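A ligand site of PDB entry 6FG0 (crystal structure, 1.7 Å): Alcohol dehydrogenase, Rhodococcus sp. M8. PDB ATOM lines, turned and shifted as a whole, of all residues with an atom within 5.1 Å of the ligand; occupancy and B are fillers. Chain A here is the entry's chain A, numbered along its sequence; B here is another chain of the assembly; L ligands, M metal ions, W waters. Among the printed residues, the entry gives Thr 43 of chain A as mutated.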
ATOM      1  N   CYS A  38     -14.424 -27.714  30.492  1.00  0.00           N
ATOM      2  CA  CYS A  38     -13.920 -26.561  29.736  1.00  0.00           C
ATOM      3  C   CYS A  38     -14.970 -26.086  28.751  1.00  0.00           C
ATOM      4  O   CYS A  38     -15.703 -26.895  28.192  1.00  0.00           O
ATOM      5  CB  CYS A  38     -12.658 -26.937  28.981  1.00  0.00           C
ATOM      6  SG  CYS A  38     -11.906 -25.575  28.002  1.00  0.00           S
ATOM      7  N   HIS A  39     -15.012 -24.783  28.480  1.00  0.00           N
ATOM      8  CA  HIS A  39     -15.957 -24.274  27.481  1.00  0.00           C
ATOM      9  C   HIS A  39     -15.723 -24.878  26.090  1.00  0.00           C
ATOM     10  O   HIS A  39     -16.658 -25.028  25.318  1.00  0.00           O
ATOM     11  CB  HIS A  39     -15.907 -22.735  27.411  1.00  0.00           C
ATOM     12  CG  HIS A  39     -17.133 -22.118  26.811  1.00  0.00           C
ATOM     13  ND1 HIS A  39     -18.012 -21.368  27.554  1.00  0.00           N
ATOM     14  CD2 HIS A  39     -17.638 -22.167  25.560  1.00  0.00           C
ATOM     15  CE1 HIS A  39     -19.008 -20.962  26.771  1.00  0.00           C
ATOM     16  NE2 HIS A  39     -18.804 -21.450  25.559  1.00  0.00           N
ATOM     17  N   SER A  40     -14.480 -25.288  25.787  1.00  0.00           N
ATOM     18  CA  SER A  40     -14.208 -26.015  24.523  1.00  0.00           C
ATOM     19  C   SER A  40     -15.099 -27.251  24.363  1.00  0.00           C
ATOM     20  O   SER A  40     -15.455 -27.626  23.245  1.00  0.00           O
ATOM     21  CB  SER A  40     -12.735 -26.396  24.417  1.00  0.00           C
ATOM     22  OG  SER A  40     -11.947 -25.238  24.289  1.00  0.00           O
ATOM     23  N   THR A  43     -18.295 -26.087  22.818  1.00  0.00           N
ATOM     24  CA  THR A  43     -18.054 -25.805  21.393  1.00  0.00           C
ATOM     25  C   THR A  43     -18.016 -27.089  20.561  1.00  0.00           C
ATOM     26  O   THR A  43     -18.703 -27.190  19.559  1.00  0.00           O
ATOM     27  CB  THR A  43     -16.767 -24.972  21.243  1.00  0.00           C
ATOM     28  OG1 THR A  43     -16.950 -23.767  22.001  1.00  0.00           O
ATOM     29  CG2 THR A  43     -16.496 -24.633  19.788  1.00  0.00           C
ATOM     30  N   ASP A 153      -5.217 -27.106  31.669  1.00  0.00           N
ATOM     31  CA  ASP A 153      -5.722 -26.350  30.516  1.00  0.00           C
ATOM     32  C   ASP A 153      -6.070 -24.910  30.893  1.00  0.00           C
ATOM     33  O   ASP A 153      -5.496 -23.975  30.307  1.00  0.00           O
ATOM     34  CB  ASP A 153      -6.873 -27.123  29.895  1.00  0.00           C
ATOM     35  CG  ASP A 153      -7.404 -26.500  28.608  1.00  0.00           C
ATOM     36  OD1 ASP A 153      -6.697 -25.747  27.901  1.00  0.00           O
ATOM     37  OD2 ASP A 153      -8.560 -26.788  28.303  1.00  0.00           O
ATOM     38  N   THR A 157      -3.017 -23.246  29.158  1.00  0.00           N
ATOM     39  CA  THR A 157      -3.286 -22.476  27.953  1.00  0.00           C
ATOM     40  C   THR A 157      -2.952 -20.976  28.117  1.00  0.00           C
ATOM     41  O   THR A 157      -2.203 -20.427  27.319  1.00  0.00           O
ATOM     42  CB  THR A 157      -4.688 -22.748  27.435  1.00  0.00           C
ATOM     43  OG1 THR A 157      -4.738 -24.132  27.102  1.00  0.00           O
ATOM     44  CG2 THR A 157      -4.998 -21.917  26.224  1.00  0.00           C
ATOM     45  N   ILE A 178      -9.283 -10.382  28.644  1.00  0.00           N
ATOM     46  CA  ILE A 178     -10.693 -10.326  28.278  1.00  0.00           C
ATOM     47  C   ILE A 178     -11.303 -11.691  28.522  1.00  0.00           C
ATOM     48  O   ILE A 178     -10.902 -12.671  27.891  1.00  0.00           O
ATOM     49  CB  ILE A 178     -10.924  -9.918  26.818  1.00  0.00           C
ATOM     50  CG1 ILE A 178     -10.163  -8.619  26.476  1.00  0.00           C
ATOM     51  CG2 ILE A 178     -12.423  -9.691  26.594  1.00  0.00           C
ATOM     52  CD1 ILE A 178     -10.353  -8.106  25.051  1.00  0.00           C
ATOM     53  N   GLY A 179     -12.297 -11.726  29.423  1.00  0.00           N
ATOM     54  CA  GLY A 179     -13.031 -12.937  29.796  1.00  0.00           C
ATOM     55  C   GLY A 179     -12.462 -13.544  31.053  1.00  0.00           C
ATOM     56  O   GLY A 179     -11.361 -14.114  31.033  1.00  0.00           O
ATOM     57  N   VAL A 180     -13.175 -13.380  32.168  1.00  0.00           N
ATOM     58  CA  VAL A 180     -12.715 -13.815  33.491  1.00  0.00           C
ATOM     59  C   VAL A 180     -13.483 -15.082  33.903  1.00  0.00           C
ATOM     60  O   VAL A 180     -14.250 -15.092  34.857  1.00  0.00           O
ATOM     61  CB  VAL A 180     -12.796 -12.690  34.530  1.00  0.00           C
ATOM     62  CG1 VAL A 180     -12.098 -13.113  35.825  1.00  0.00           C
ATOM     63  CG2 VAL A 180     -12.206 -11.405  33.969  1.00  0.00           C
ATOM     64  N   GLY A 181     -13.259 -16.129  33.137  1.00  0.00           N
ATOM     65  CA  GLY A 181     -13.848 -17.434  33.402  1.00  0.00           C
ATOM     66  C   GLY A 181     -12.775 -18.392  33.824  1.00  0.00           C
ATOM     67  O   GLY A 181     -11.842 -18.020  34.526  1.00  0.00           O
ATOM     68  N   GLY A 182     -12.936 -19.647  33.431  1.00  0.00           N
ATOM     69  CA  GLY A 182     -11.989 -20.691  33.766  1.00  0.00           C
ATOM     70  C   GLY A 182     -10.564 -20.292  33.441  1.00  0.00           C
ATOM     71  O   GLY A 182      -9.717 -20.207  34.352  1.00  0.00           O
ATOM     72  N   LEU A 183     -10.295 -19.999  32.182  1.00  0.00           N
ATOM     73  CA  LEU A 183      -8.967 -19.598  31.735  1.00  0.00           C
ATOM     74  C   LEU A 183      -8.576 -18.221  32.268  1.00  0.00           C
ATOM     75  O   LEU A 183      -7.477 -18.043  32.810  1.00  0.00           O
ATOM     76  CB  LEU A 183      -8.854 -19.591  30.199  1.00  0.00           C
ATOM     77  CG  LEU A 183      -8.427 -20.901  29.557  1.00  0.00           C
ATOM     78  CD1 LEU A 183      -9.486 -22.005  29.711  1.00  0.00           C
ATOM     79  CD2 LEU A 183      -8.076 -20.677  28.102  1.00  0.00           C
ATOM     80  N   GLY A 184      -9.457 -17.250  32.074  1.00  0.00           N
ATOM     81  CA  GLY A 184      -9.105 -15.864  32.376  1.00  0.00           C
ATOM     82  C   GLY A 184      -8.751 -15.583  33.820  1.00  0.00           C
ATOM     83  O   GLY A 184      -7.817 -14.805  34.098  1.00  0.00           O
ATOM     84  N   VAL A 202     -11.472  -7.550  31.842  1.00  0.00           N
ATOM     85  CA  VAL A 202     -12.641  -7.106  31.064  1.00  0.00           C
ATOM     86  C   VAL A 202     -13.617  -8.264  31.031  1.00  0.00           C
ATOM     87  O   VAL A 202     -13.223  -9.389  30.710  1.00  0.00           O
ATOM     88  CB  VAL A 202     -12.232  -6.723  29.619  1.00  0.00           C
ATOM     89  CG1 VAL A 202     -13.446  -6.283  28.778  1.00  0.00           C
ATOM     90  CG2 VAL A 202     -11.156  -5.641  29.644  1.00  0.00           C
ATOM     91  N   ASP A 203     -14.872  -7.994  31.397  1.00  0.00           N
ATOM     92  CA  ASP A 203     -15.927  -9.022  31.340  1.00  0.00           C
ATOM     93  C   ASP A 203     -17.278  -8.338  31.182  1.00  0.00           C
ATOM     94  O   ASP A 203     -17.420  -7.137  31.482  1.00  0.00           O
ATOM     95  CB  ASP A 203     -15.902  -9.932  32.569  1.00  0.00           C
ATOM     96  CG  ASP A 203     -16.519 -11.328  32.294  1.00  0.00           C
ATOM     97  OD1 ASP A 203     -17.764 -11.407  32.112  1.00  0.00           O
ATOM     98  OD2 ASP A 203     -15.749 -12.330  32.287  1.00  0.00           O
ATOM     99  N   LEU A 204     -18.260  -9.079  30.665  1.00  0.00           N
ATOM    100  CA  LEU A 204     -19.627  -8.578  30.576  1.00  0.00           C
ATOM    101  C   LEU A 204     -20.332  -8.518  31.936  1.00  0.00           C
ATOM    102  O   LEU A 204     -21.243  -7.721  32.124  1.00  0.00           O
ATOM    103  CB  LEU A 204     -20.482  -9.465  29.653  1.00  0.00           C
ATOM    104  CG  LEU A 204     -20.134  -9.430  28.173  1.00  0.00           C
ATOM    105  CD1 LEU A 204     -20.852 -10.577  27.455  1.00  0.00           C
ATOM    106  CD2 LEU A 204     -20.555  -8.089  27.603  1.00  0.00           C
ATOM    107  N   ASP A 205     -19.902  -9.371  32.849  1.00  0.00           N
ATOM    108  CA  ASP A 205     -20.627  -9.629  34.086  1.00  0.00           C
ATOM    109  C   ASP A 205     -19.890  -8.949  35.258  1.00  0.00           C
ATOM    110  O   ASP A 205     -18.703  -9.235  35.485  1.00  0.00           O
ATOM    111  CB  ASP A 205     -20.701 -11.159  34.244  1.00  0.00           C
ATOM    112  CG  ASP A 205     -21.434 -11.618  35.489  1.00  0.00           C
ATOM    113  OD1 ASP A 205     -21.570 -10.859  36.465  1.00  0.00           O
ATOM    114  OD2 ASP A 205     -21.888 -12.793  35.527  1.00  0.00           O
ATOM    115  N   ARG A 208     -18.074 -11.218  37.577  1.00  0.00           N
ATOM    116  CA  ARG A 208     -16.780 -11.684  37.050  1.00  0.00           C
ATOM    117  C   ARG A 208     -15.714 -10.608  37.172  1.00  0.00           C
ATOM    118  O   ARG A 208     -14.545 -10.918  37.350  1.00  0.00           O
ATOM    119  CB  ARG A 208     -16.899 -12.188  35.618  1.00  0.00           C
ATOM    120  CG  ARG A 208     -17.873 -13.346  35.419  1.00  0.00           C
ATOM    121  CD  ARG A 208     -17.519 -14.533  36.255  1.00  0.00           C
ATOM    122  NE  ARG A 208     -18.484 -15.626  36.104  1.00  0.00           N
ATOM    123  CZ  ARG A 208     -18.311 -16.737  35.404  1.00  0.00           C
ATOM    124  NH1 ARG A 208     -17.204 -16.999  34.759  1.00  0.00           N
ATOM    125  NH2 ARG A 208     -19.288 -17.659  35.408  1.00  0.00           N
ATOM    126  N   SER A 223     -17.044  -5.026  29.554  1.00  0.00           N
ATOM    127  CA  SER A 223     -16.861  -5.299  28.140  1.00  0.00           C
ATOM    128  C   SER A 223     -17.965  -4.622  27.319  1.00  0.00           C
ATOM    129  O   SER A 223     -18.985  -4.203  27.866  1.00  0.00           O
ATOM    130  CB  SER A 223     -16.900  -6.801  27.876  1.00  0.00           C
ATOM    131  OG  SER A 223     -16.344  -7.108  26.614  1.00  0.00           O
ATOM    132  N   PHE A 246      -9.509 -14.130  25.967  1.00  0.00           N
ATOM    133  CA  PHE A 246     -10.040 -15.474  26.287  1.00  0.00           C
ATOM    134  C   PHE A 246     -11.476 -15.650  25.860  1.00  0.00           C
ATOM    135  O   PHE A 246     -12.104 -16.667  26.192  1.00  0.00           O
ATOM    136  CB  PHE A 246      -9.851 -15.789  27.768  1.00  0.00           C
ATOM    137  CG  PHE A 246      -8.415 -15.765  28.177  1.00  0.00           C
ATOM    138  CD1 PHE A 246      -7.554 -16.807  27.786  1.00  0.00           C
ATOM    139  CD2 PHE A 246      -7.889 -14.717  28.914  1.00  0.00           C
ATOM    140  CE1 PHE A 246      -6.220 -16.780  28.115  1.00  0.00           C
ATOM    141  CE2 PHE A 246      -6.534 -14.698  29.265  1.00  0.00           C
ATOM    142  CZ  PHE A 246      -5.715 -15.731  28.876  1.00  0.00           C
ATOM    143  N   VAL A 247     -12.037 -14.678  25.144  1.00  0.00           N
ATOM    144  CA  VAL A 247     -13.382 -14.813  24.573  1.00  0.00           C
ATOM    145  C   VAL A 247     -13.256 -15.093  23.068  1.00  0.00           C
ATOM    146  O   VAL A 247     -13.793 -16.093  22.551  1.00  0.00           O
ATOM    147  CB  VAL A 247     -14.221 -13.528  24.800  1.00  0.00           C
ATOM    148  CG1 VAL A 247     -15.621 -13.678  24.207  1.00  0.00           C
ATOM    149  CG2 VAL A 247     -14.339 -13.205  26.290  1.00  0.00           C
ATOM    150  N   SER A 251     -16.325  -8.923  18.597  1.00  0.00           N
ATOM    151  CA  SER A 251     -16.376  -7.663  19.371  1.00  0.00           C
ATOM    152  C   SER A 251     -15.161  -7.526  20.294  1.00  0.00           C
ATOM    153  O   SER A 251     -14.617  -6.427  20.431  1.00  0.00           O
ATOM    154  CB  SER A 251     -17.675  -7.570  20.191  1.00  0.00           C
ATOM    155  OG  SER A 251     -17.805  -8.658  21.059  1.00  0.00           O
ATOM    156  N   THR A 252     -14.713  -8.635  20.893  1.00  0.00           N
ATOM    157  CA  THR A 252     -13.571  -8.598  21.800  1.00  0.00           C
ATOM    158  C   THR A 252     -12.254  -8.456  21.059  1.00  0.00           C
ATOM    159  O   THR A 252     -11.349  -7.760  21.527  1.00  0.00           O
ATOM    160  CB  THR A 252     -13.528  -9.816  22.756  1.00  0.00           C
ATOM    161  OG1 THR A 252     -13.471 -11.040  22.012  1.00  0.00           O
ATOM    162  CG2 THR A 252     -14.742  -9.825  23.676  1.00  0.00           C
ATOM    163  N   VAL A 269      -7.077 -16.262  22.184  1.00  0.00           N
ATOM    164  CA  VAL A 269      -7.092 -17.569  22.841  1.00  0.00           C
ATOM    165  C   VAL A 269      -8.488 -18.166  22.780  1.00  0.00           C
ATOM    166  O   VAL A 269      -8.640 -19.350  22.489  1.00  0.00           O
ATOM    167  CB  VAL A 269      -6.626 -17.461  24.309  1.00  0.00           C
ATOM    168  CG1 VAL A 269      -6.576 -18.831  24.972  1.00  0.00           C
ATOM    169  CG2 VAL A 269      -5.284 -16.735  24.379  1.00  0.00           C
ATOM    170  N   GLY A 270      -9.514 -17.363  23.081  1.00  0.00           N
ATOM    171  CA  GLY A 270     -10.882 -17.819  22.975  1.00  0.00           C
ATOM    172  C   GLY A 270     -11.250 -18.171  21.538  1.00  0.00           C
ATOM    173  O   GLY A 270     -10.728 -17.555  20.593  1.00  0.00           O
ATOM    174  N   ILE A 271     -12.141 -19.157  21.392  1.00  0.00           N
ATOM    175  CA  ILE A 271     -12.476 -19.736  20.107  1.00  0.00           C
ATOM    176  C   ILE A 271     -13.954 -19.463  19.796  1.00  0.00           C
ATOM    177  O   ILE A 271     -14.861 -19.963  20.481  1.00  0.00           O
ATOM    178  CB  ILE A 271     -12.191 -21.261  20.081  1.00  0.00           C
ATOM    179  CG1 ILE A 271     -10.687 -21.520  20.336  1.00  0.00           C
ATOM    180  CG2 ILE A 271     -12.644 -21.884  18.762  1.00  0.00           C
ATOM    181  CD1 ILE A 271     -10.346 -22.965  20.721  1.00  0.00           C
ATOM    182  N   PRO A 293      -2.821 -18.972  19.851  1.00  0.00           N
ATOM    183  CA  PRO A 293      -2.017 -20.046  20.427  1.00  0.00           C
ATOM    184  C   PRO A 293      -2.870 -21.270  20.693  1.00  0.00           C
ATOM    185  O   PRO A 293      -4.105 -21.149  20.694  1.00  0.00           O
ATOM    186  CB  PRO A 293      -1.494 -19.419  21.710  1.00  0.00           C
ATOM    187  CG  PRO A 293      -2.595 -18.511  22.138  1.00  0.00           C
ATOM    188  CD  PRO A 293      -3.208 -17.985  20.887  1.00  0.00           C
ATOM    189  N   TYR A 294      -2.242 -22.423  20.893  1.00  0.00           N
ATOM    190  CA  TYR A 294      -2.956 -23.657  21.178  1.00  0.00           C
ATOM    191  C   TYR A 294      -2.321 -24.373  22.372  1.00  0.00           C
ATOM    192  O   TYR A 294      -1.167 -24.743  22.321  1.00  0.00           O
ATOM    193  CB  TYR A 294      -2.906 -24.578  19.980  1.00  0.00           C
ATOM    194  CG  TYR A 294      -3.469 -25.970  20.227  1.00  0.00           C
ATOM    195  CD1 TYR A 294      -4.787 -26.161  20.621  1.00  0.00           C
ATOM    196  CD2 TYR A 294      -2.691 -27.095  20.045  1.00  0.00           C
ATOM    197  CE1 TYR A 294      -5.304 -27.442  20.815  1.00  0.00           C
ATOM    198  CE2 TYR A 294      -3.185 -28.392  20.230  1.00  0.00           C
ATOM    199  CZ  TYR A 294      -4.492 -28.557  20.624  1.00  0.00           C
ATOM    200  OH  TYR A 294      -4.981 -29.848  20.821  1.00  0.00           O
ATOM    201  N   TRP A 295      -3.130 -24.520  23.431  1.00  0.00           N
ATOM    202  CA  TRP A 295      -2.789 -25.333  24.597  1.00  0.00           C
ATOM    203  C   TRP A 295      -1.405 -24.924  25.140  1.00  0.00           C
ATOM    204  O   TRP A 295      -1.173 -23.733  25.299  1.00  0.00           O
ATOM    205  CB  TRP A 295      -2.974 -26.815  24.287  1.00  0.00           C
ATOM    206  CG  TRP A 295      -3.562 -27.605  25.453  1.00  0.00           C
ATOM    207  CD1 TRP A 295      -3.421 -27.344  26.770  1.00  0.00           C
ATOM    208  CD2 TRP A 295      -4.362 -28.786  25.358  1.00  0.00           C
ATOM    209  NE1 TRP A 295      -4.108 -28.289  27.519  1.00  0.00           N
ATOM    210  CE2 TRP A 295      -4.693 -29.176  26.662  1.00  0.00           C
ATOM    211  CE3 TRP A 295      -4.840 -29.538  24.282  1.00  0.00           C
ATOM    212  CZ2 TRP A 295      -5.488 -30.287  26.935  1.00  0.00           C
ATOM    213  CZ3 TRP A 295      -5.601 -30.640  24.547  1.00  0.00           C
ATOM    214  CH2 TRP A 295      -5.918 -31.012  25.854  1.00  0.00           C
ATOM    215  N   LEU A 332     -22.286 -24.566  32.937  1.00  0.00           N
ATOM    216  CA  LEU A 332     -21.238 -23.908  32.166  1.00  0.00           C
ATOM    217  C   LEU A 332     -21.841 -23.159  30.970  1.00  0.00           C
ATOM    218  O   LEU A 332     -21.478 -22.015  30.707  1.00  0.00           O
ATOM    219  CB  LEU A 332     -20.181 -24.913  31.701  1.00  0.00           C
ATOM    220  CG  LEU A 332     -18.935 -24.319  31.052  1.00  0.00           C
ATOM    221  CD1 LEU A 332     -18.204 -23.391  32.035  1.00  0.00           C
ATOM    222  CD2 LEU A 332     -18.040 -25.456  30.570  1.00  0.00           C
ATOM    223  N   GLY A 339     -15.673 -19.597  37.949  1.00  0.00           N
ATOM    224  CA  GLY A 339     -14.368 -20.224  37.831  1.00  0.00           C
ATOM    225  C   GLY A 339     -14.499 -21.518  37.025  1.00  0.00           C
ATOM    226  O   GLY A 339     -15.092 -21.518  35.949  1.00  0.00           O
ATOM    227  N   ARG A 340     -13.964 -22.614  37.561  1.00  0.00           N
ATOM    228  CA  ARG A 340     -13.920 -23.902  36.877  1.00  0.00           C
ATOM    229  C   ARG A 340     -14.793 -24.940  37.524  1.00  0.00           C
ATOM    230  O   ARG A 340     -14.736 -25.155  38.751  1.00  0.00           O
ATOM    231  CB  ARG A 340     -12.491 -24.464  36.849  1.00  0.00           C
ATOM    232  CG  ARG A 340     -11.801 -24.298  35.512  1.00  0.00           C
ATOM    233  CD  ARG A 340     -12.348 -25.283  34.522  1.00  0.00           C
ATOM    234  NE  ARG A 340     -11.503 -25.400  33.335  1.00  0.00           N
ATOM    235  CZ  ARG A 340     -11.652 -24.746  32.182  1.00  0.00           C
ATOM    236  NH1 ARG A 340     -12.593 -23.812  32.012  1.00  0.00           N
ATOM    237  NH2 ARG A 340     -10.833 -25.022  31.188  1.00  0.00           N
ATOM    238  N   PHE B 281      -9.091 -18.755  14.509  1.00  0.00           N
ATOM    239  CA  PHE B 281      -9.132 -20.212  14.480  1.00  0.00           C
ATOM    240  C   PHE B 281      -9.767 -20.704  13.190  1.00  0.00           C
ATOM    241  O   PHE B 281     -10.731 -20.084  12.675  1.00  0.00           O
ATOM    242  CB  PHE B 281      -9.851 -20.745  15.722  1.00  0.00           C
ATOM    243  CG  PHE B 281      -9.045 -20.564  16.964  1.00  0.00           C
ATOM    244  CD1 PHE B 281      -8.056 -21.496  17.322  1.00  0.00           C
ATOM    245  CD2 PHE B 281      -9.183 -19.415  17.740  1.00  0.00           C
ATOM    246  CE1 PHE B 281      -7.285 -21.308  18.458  1.00  0.00           C
ATOM    247  CE2 PHE B 281      -8.412 -19.226  18.876  1.00  0.00           C
ATOM    248  CZ  PHE B 281      -7.452 -20.169  19.234  1.00  0.00           C
HETATM  249  P1  LIG L   1     -15.801 -19.992  30.591  1.00  0.00           P
HETATM  250  O1  LIG L   1     -17.183 -20.311  30.045  1.00  0.00           O
HETATM  251  O2  LIG L   1     -15.326 -20.540  31.896  1.00  0.00           O
HETATM  252  O3  LIG L   1     -15.709 -18.404  30.720  1.00  0.00           O
HETATM  253  C1  LIG L   1     -16.271 -17.468  29.833  1.00  0.00           C
HETATM  254  C2  LIG L   1     -16.030 -16.064  30.415  1.00  0.00           C
HETATM  255  O4  LIG L   1     -15.990 -15.150  29.325  1.00  0.00           O
HETATM  256  C3  LIG L   1     -17.109 -15.617  31.408  1.00  0.00           C
HETATM  257  O5  LIG L   1     -16.554 -14.964  32.568  1.00  0.00           O
HETATM  258  C4  LIG L   1     -17.975 -14.699  30.541  1.00  0.00           C
HETATM  259  O6  LIG L   1     -18.798 -13.766  31.235  1.00  0.00           O
HETATM  260  C5  LIG L   1     -16.884 -14.080  29.675  1.00  0.00           C
HETATM  261  N1  LIG L   1     -17.345 -13.447  28.440  1.00  0.00           N
HETATM  262  C6  LIG L   1     -18.249 -13.980  27.557  1.00  0.00           C
HETATM  263  N2  LIG L   1     -18.452 -13.117  26.555  1.00  0.00           N
HETATM  264  C7  LIG L   1     -17.720 -12.009  26.809  1.00  0.00           C
HETATM  265  C8  LIG L   1     -17.484 -10.713  26.142  1.00  0.00           C
HETATM  266  N3  LIG L   1     -18.087 -10.405  24.998  1.00  0.00           N
HETATM  267  N4  LIG L   1     -16.638  -9.827  26.706  1.00  0.00           N
HETATM  268  C9  LIG L   1     -16.011 -10.137  27.851  1.00  0.00           C
HETATM  269  N5  LIG L   1     -16.168 -11.274  28.537  1.00  0.00           N
HETATM  270  C10 LIG L   1     -17.000 -12.227  28.057  1.00  0.00           C
HETATM  271  O7  LIG L   1     -14.792 -20.311  29.390  1.00  0.00           O
HETATM  272  P2  LIG L   1     -13.369 -21.016  29.506  1.00  0.00           P
HETATM  273  O8  LIG L   1     -13.540 -22.471  29.796  1.00  0.00           O
HETATM  274  O9  LIG L   1     -12.425 -20.156  30.352  1.00  0.00           O
HETATM  275  O10 LIG L   1     -12.885 -20.889  27.983  1.00  0.00           O
HETATM  276  C11 LIG L   1     -12.648 -19.617  27.376  1.00  0.00           C
HETATM  277  C12 LIG L   1     -12.375 -19.749  25.879  1.00  0.00           C
HETATM  278  O11 LIG L   1     -11.038 -20.258  25.679  1.00  0.00           O
HETATM  279  C13 LIG L   1     -13.323 -20.662  25.118  1.00  0.00           C
HETATM  280  O12 LIG L   1     -13.579 -20.132  23.815  1.00  0.00           O
HETATM  281  C14 LIG L   1     -12.509 -21.931  24.966  1.00  0.00           C
HETATM  282  O13 LIG L   1     -12.972 -22.757  23.887  1.00  0.00           O
HETATM  283  C15 LIG L   1     -11.127 -21.340  24.756  1.00  0.00           C
HETATM  284  N6  LIG L   1      -9.977 -22.235  24.947  1.00  0.00           N
HETATM  285  C16 LIG L   1      -8.978 -22.141  24.049  1.00  0.00           C
HETATM  286  C17 LIG L   1      -7.862 -22.953  24.122  1.00  0.00           C
HETATM  287  C18 LIG L   1      -6.727 -22.814  23.145  1.00  0.00           C
HETATM  288  O14 LIG L   1      -5.828 -23.646  23.135  1.00  0.00           O
HETATM  289  N7  LIG L   1      -6.609 -21.721  22.370  1.00  0.00           N
HETATM  290  C19 LIG L   1      -7.763 -23.883  25.177  1.00  0.00           C
HETATM  291  C20 LIG L   1      -8.783 -23.923  26.123  1.00  0.00           C
HETATM  292  C21 LIG L   1      -9.881 -23.087  25.999  1.00  0.00           C
HETATM  293 ZN    ZN M   1     -10.140 -26.848  27.214  1.00  0.00          ZN
HETATM  294  O   HOH W   1     -20.135 -11.919  23.466  1.00  0.00           O
HETATM  295  O   HOH W   2     -19.491 -20.143  31.275  1.00  0.00           O
HETATM  296  O   HOH W   3     -21.273 -13.264  30.414  1.00  0.00           O
HETATM  297  O   HOH W   4     -13.376 -16.173  28.610  1.00  0.00           O
HETATM  298  O   HOH W   5     -15.141 -17.892  23.923  1.00  0.00           O
HETATM  299  O   HOH W   6     -16.619 -19.770  34.157  1.00  0.00           O
HETATM  300  O   HOH W   7     -17.843  -7.678  23.684  1.00  0.00           O
HETATM  301  O   HOH W   8     -19.613 -14.343  24.331  1.00  0.00           O
HETATM  302  O   HOH W   9     -14.896 -22.661  33.466  1.00  0.00           O
HETATM  303  O   HOH W  10     -19.345 -17.236  27.679  1.00  0.00           O
HETATM  304  O   HOH W  11     -12.061 -17.536  30.718  1.00  0.00           O
HETATM  305  O   HOH W  12     -14.854 -22.321  22.146  1.00  0.00           O
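OG of Ser 40 sits at hydrogen-bond distance from O13 of the ligand, at 2.7 Å.
OD1 of Asp 203 is in hydrogen-bond range of O6 of the ligand.
The side-chain hydroxyl (OG) of Ser 223 is in hydrogen-bond range of a nitrogen (N4) of the ligand, 2.7 Å away.
The guanidinium group of Arg 340 lies within salt-bridge range of an oxygen (O8) of the ligand.
The backbone NH (N) of Leu 183 is in hydrogen-bond range of an oxygen (O9) of the ligand, at 2.8 Å.
The backbone NH (N) of His 39 lies within hydrogen-bond range of an oxygen (O8) of the ligand (3.0 Å).
ND1 of His 39 is in hydrogen-bond range of O1 of the ligand (2.8 Å).
N of Trp 295 lies within hydrogen-bond range of O14 of the ligand.
N of Gly 182 lies within hydrogen-bond range of O2 of the ligand.
O12 of the ligand sits at hydrogen-bond distance from N of Ile 271 (3.0 Å).
An oxygen (O5) of the ligand is in hydrogen-bond range of the guanidinium group (NH1) of Arg 208, 3.1 Å away.
O of Pro 293 lies within hydrogen-bond range of N7 of the ligand, at 3.1 Å.
N7 of the ligand is in hydrogen-bond range of O of Val 269 (3.1 Å).
The backbone carbonyl oxygen (O) of Val 180 is in hydrogen-bond range of an oxygen (O5) of the ligand (3.3 Å).
The backbone NH of Ser 40 sits close to the side-chain sulfur of Cys 38 (3.4 Å).
O of Asp 203 sits at hydrogen-bond distance from N of Ser 223, at 2.9 Å.
The side-chain carboxylate of Asp 203 lies within hydrogen-bond range of the backbone NH of Val 180, at 2.8 Å.
OD1 of Asp 203 lies within hydrogen-bond range of N of Asp 205, 3.0 Å away.
The guanidinium group (NH2) of Arg 340 lies close to the side-chain sulfur (SG) of Cys 38 (3.4 Å).
O of Ile 178 lies within hydrogen-bond range of N of Phe 246 (2.8 Å).
The side-chain carboxylate (OD1) of Asp 153 sits at hydrogen-bond distance from the side-chain hydroxyl (OG1) of Thr 157 (2.7 Å).
O of Val 202 is in hydrogen-bond range of N of Gly 179, 2.8 Å away.
SG of Cys 38 touches C21 of the ligand, at 3.8 Å.
Asp 153 touches the ligand (OD1 to C20, 3.3 Å).
CG2 of Thr 157 touches C19 of the ligand (3.6 Å).
Ile 178 touches the ligand (CG2 to C9, 3.8 Å).
Gly 179 touches the ligand.
Gly 181 touches the ligand (CA to O3, 3.4 Å).
CD1 of Leu 204 touches C7 of the ligand (3.5 Å).
Phe 246 touches the ligand (O to C12, 3.1 Å).
Val 247 touches the ligand (CG2 to C10, 3.3 Å).
Thr 252 touches the ligand (CG2 to N4, 3.6 Å).
CA of Gly 270 touches O11 of the ligand, 3.6 Å away.
Tyr 294 touches the ligand (CA to O14, 3.5 Å).
Leu 332 touches the ligand (CD1 to O1, 3.8 Å).
CZ of Phe 281 of chain B touches N7 of the ligand (3.6 Å).
Hydrophobic or aromatic side chains within 4 Å of the ligand: His 39, Ile 178, Leu 183, Leu 204, Val 247, Val 269, Ile 271, Tyr 294, Leu 332 and Phe 281 of chain B.
The nearest printed residue that does not touch the ligand is Val 202 (4.1 Å).
Water W12 lies within hydrogen-bond range of the side-chain hydroxyl (OG1) of Thr 43, an oxygen (O13) of the ligand and the backbone carbonyl oxygen (O) of Ile 271.
Water W2 lies within hydrogen-bond range of O1 of the ligand and O of Leu 332.
Water W6 lies within hydrogen-bond range of O2 of the ligand (2.7 Å), NH1 of Arg 208 (2.9 Å) and O of Gly 339 (2.9 Å).
Water W5 bridges O of Val 247 (2.6 Å) and O12 of the ligand (2.7 Å).
Water W4 lies within hydrogen-bond range of O of Phe 246 (2.8 Å) and O4 of the ligand (2.9 Å).
Water W7 lies within hydrogen-bond range of the side-chain hydroxyl of Ser 251 (2.8 Å), a nitrogen (N3) of the ligand (3.0 Å) and the side-chain hydroxyl of Ser 223 (3.3 Å).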
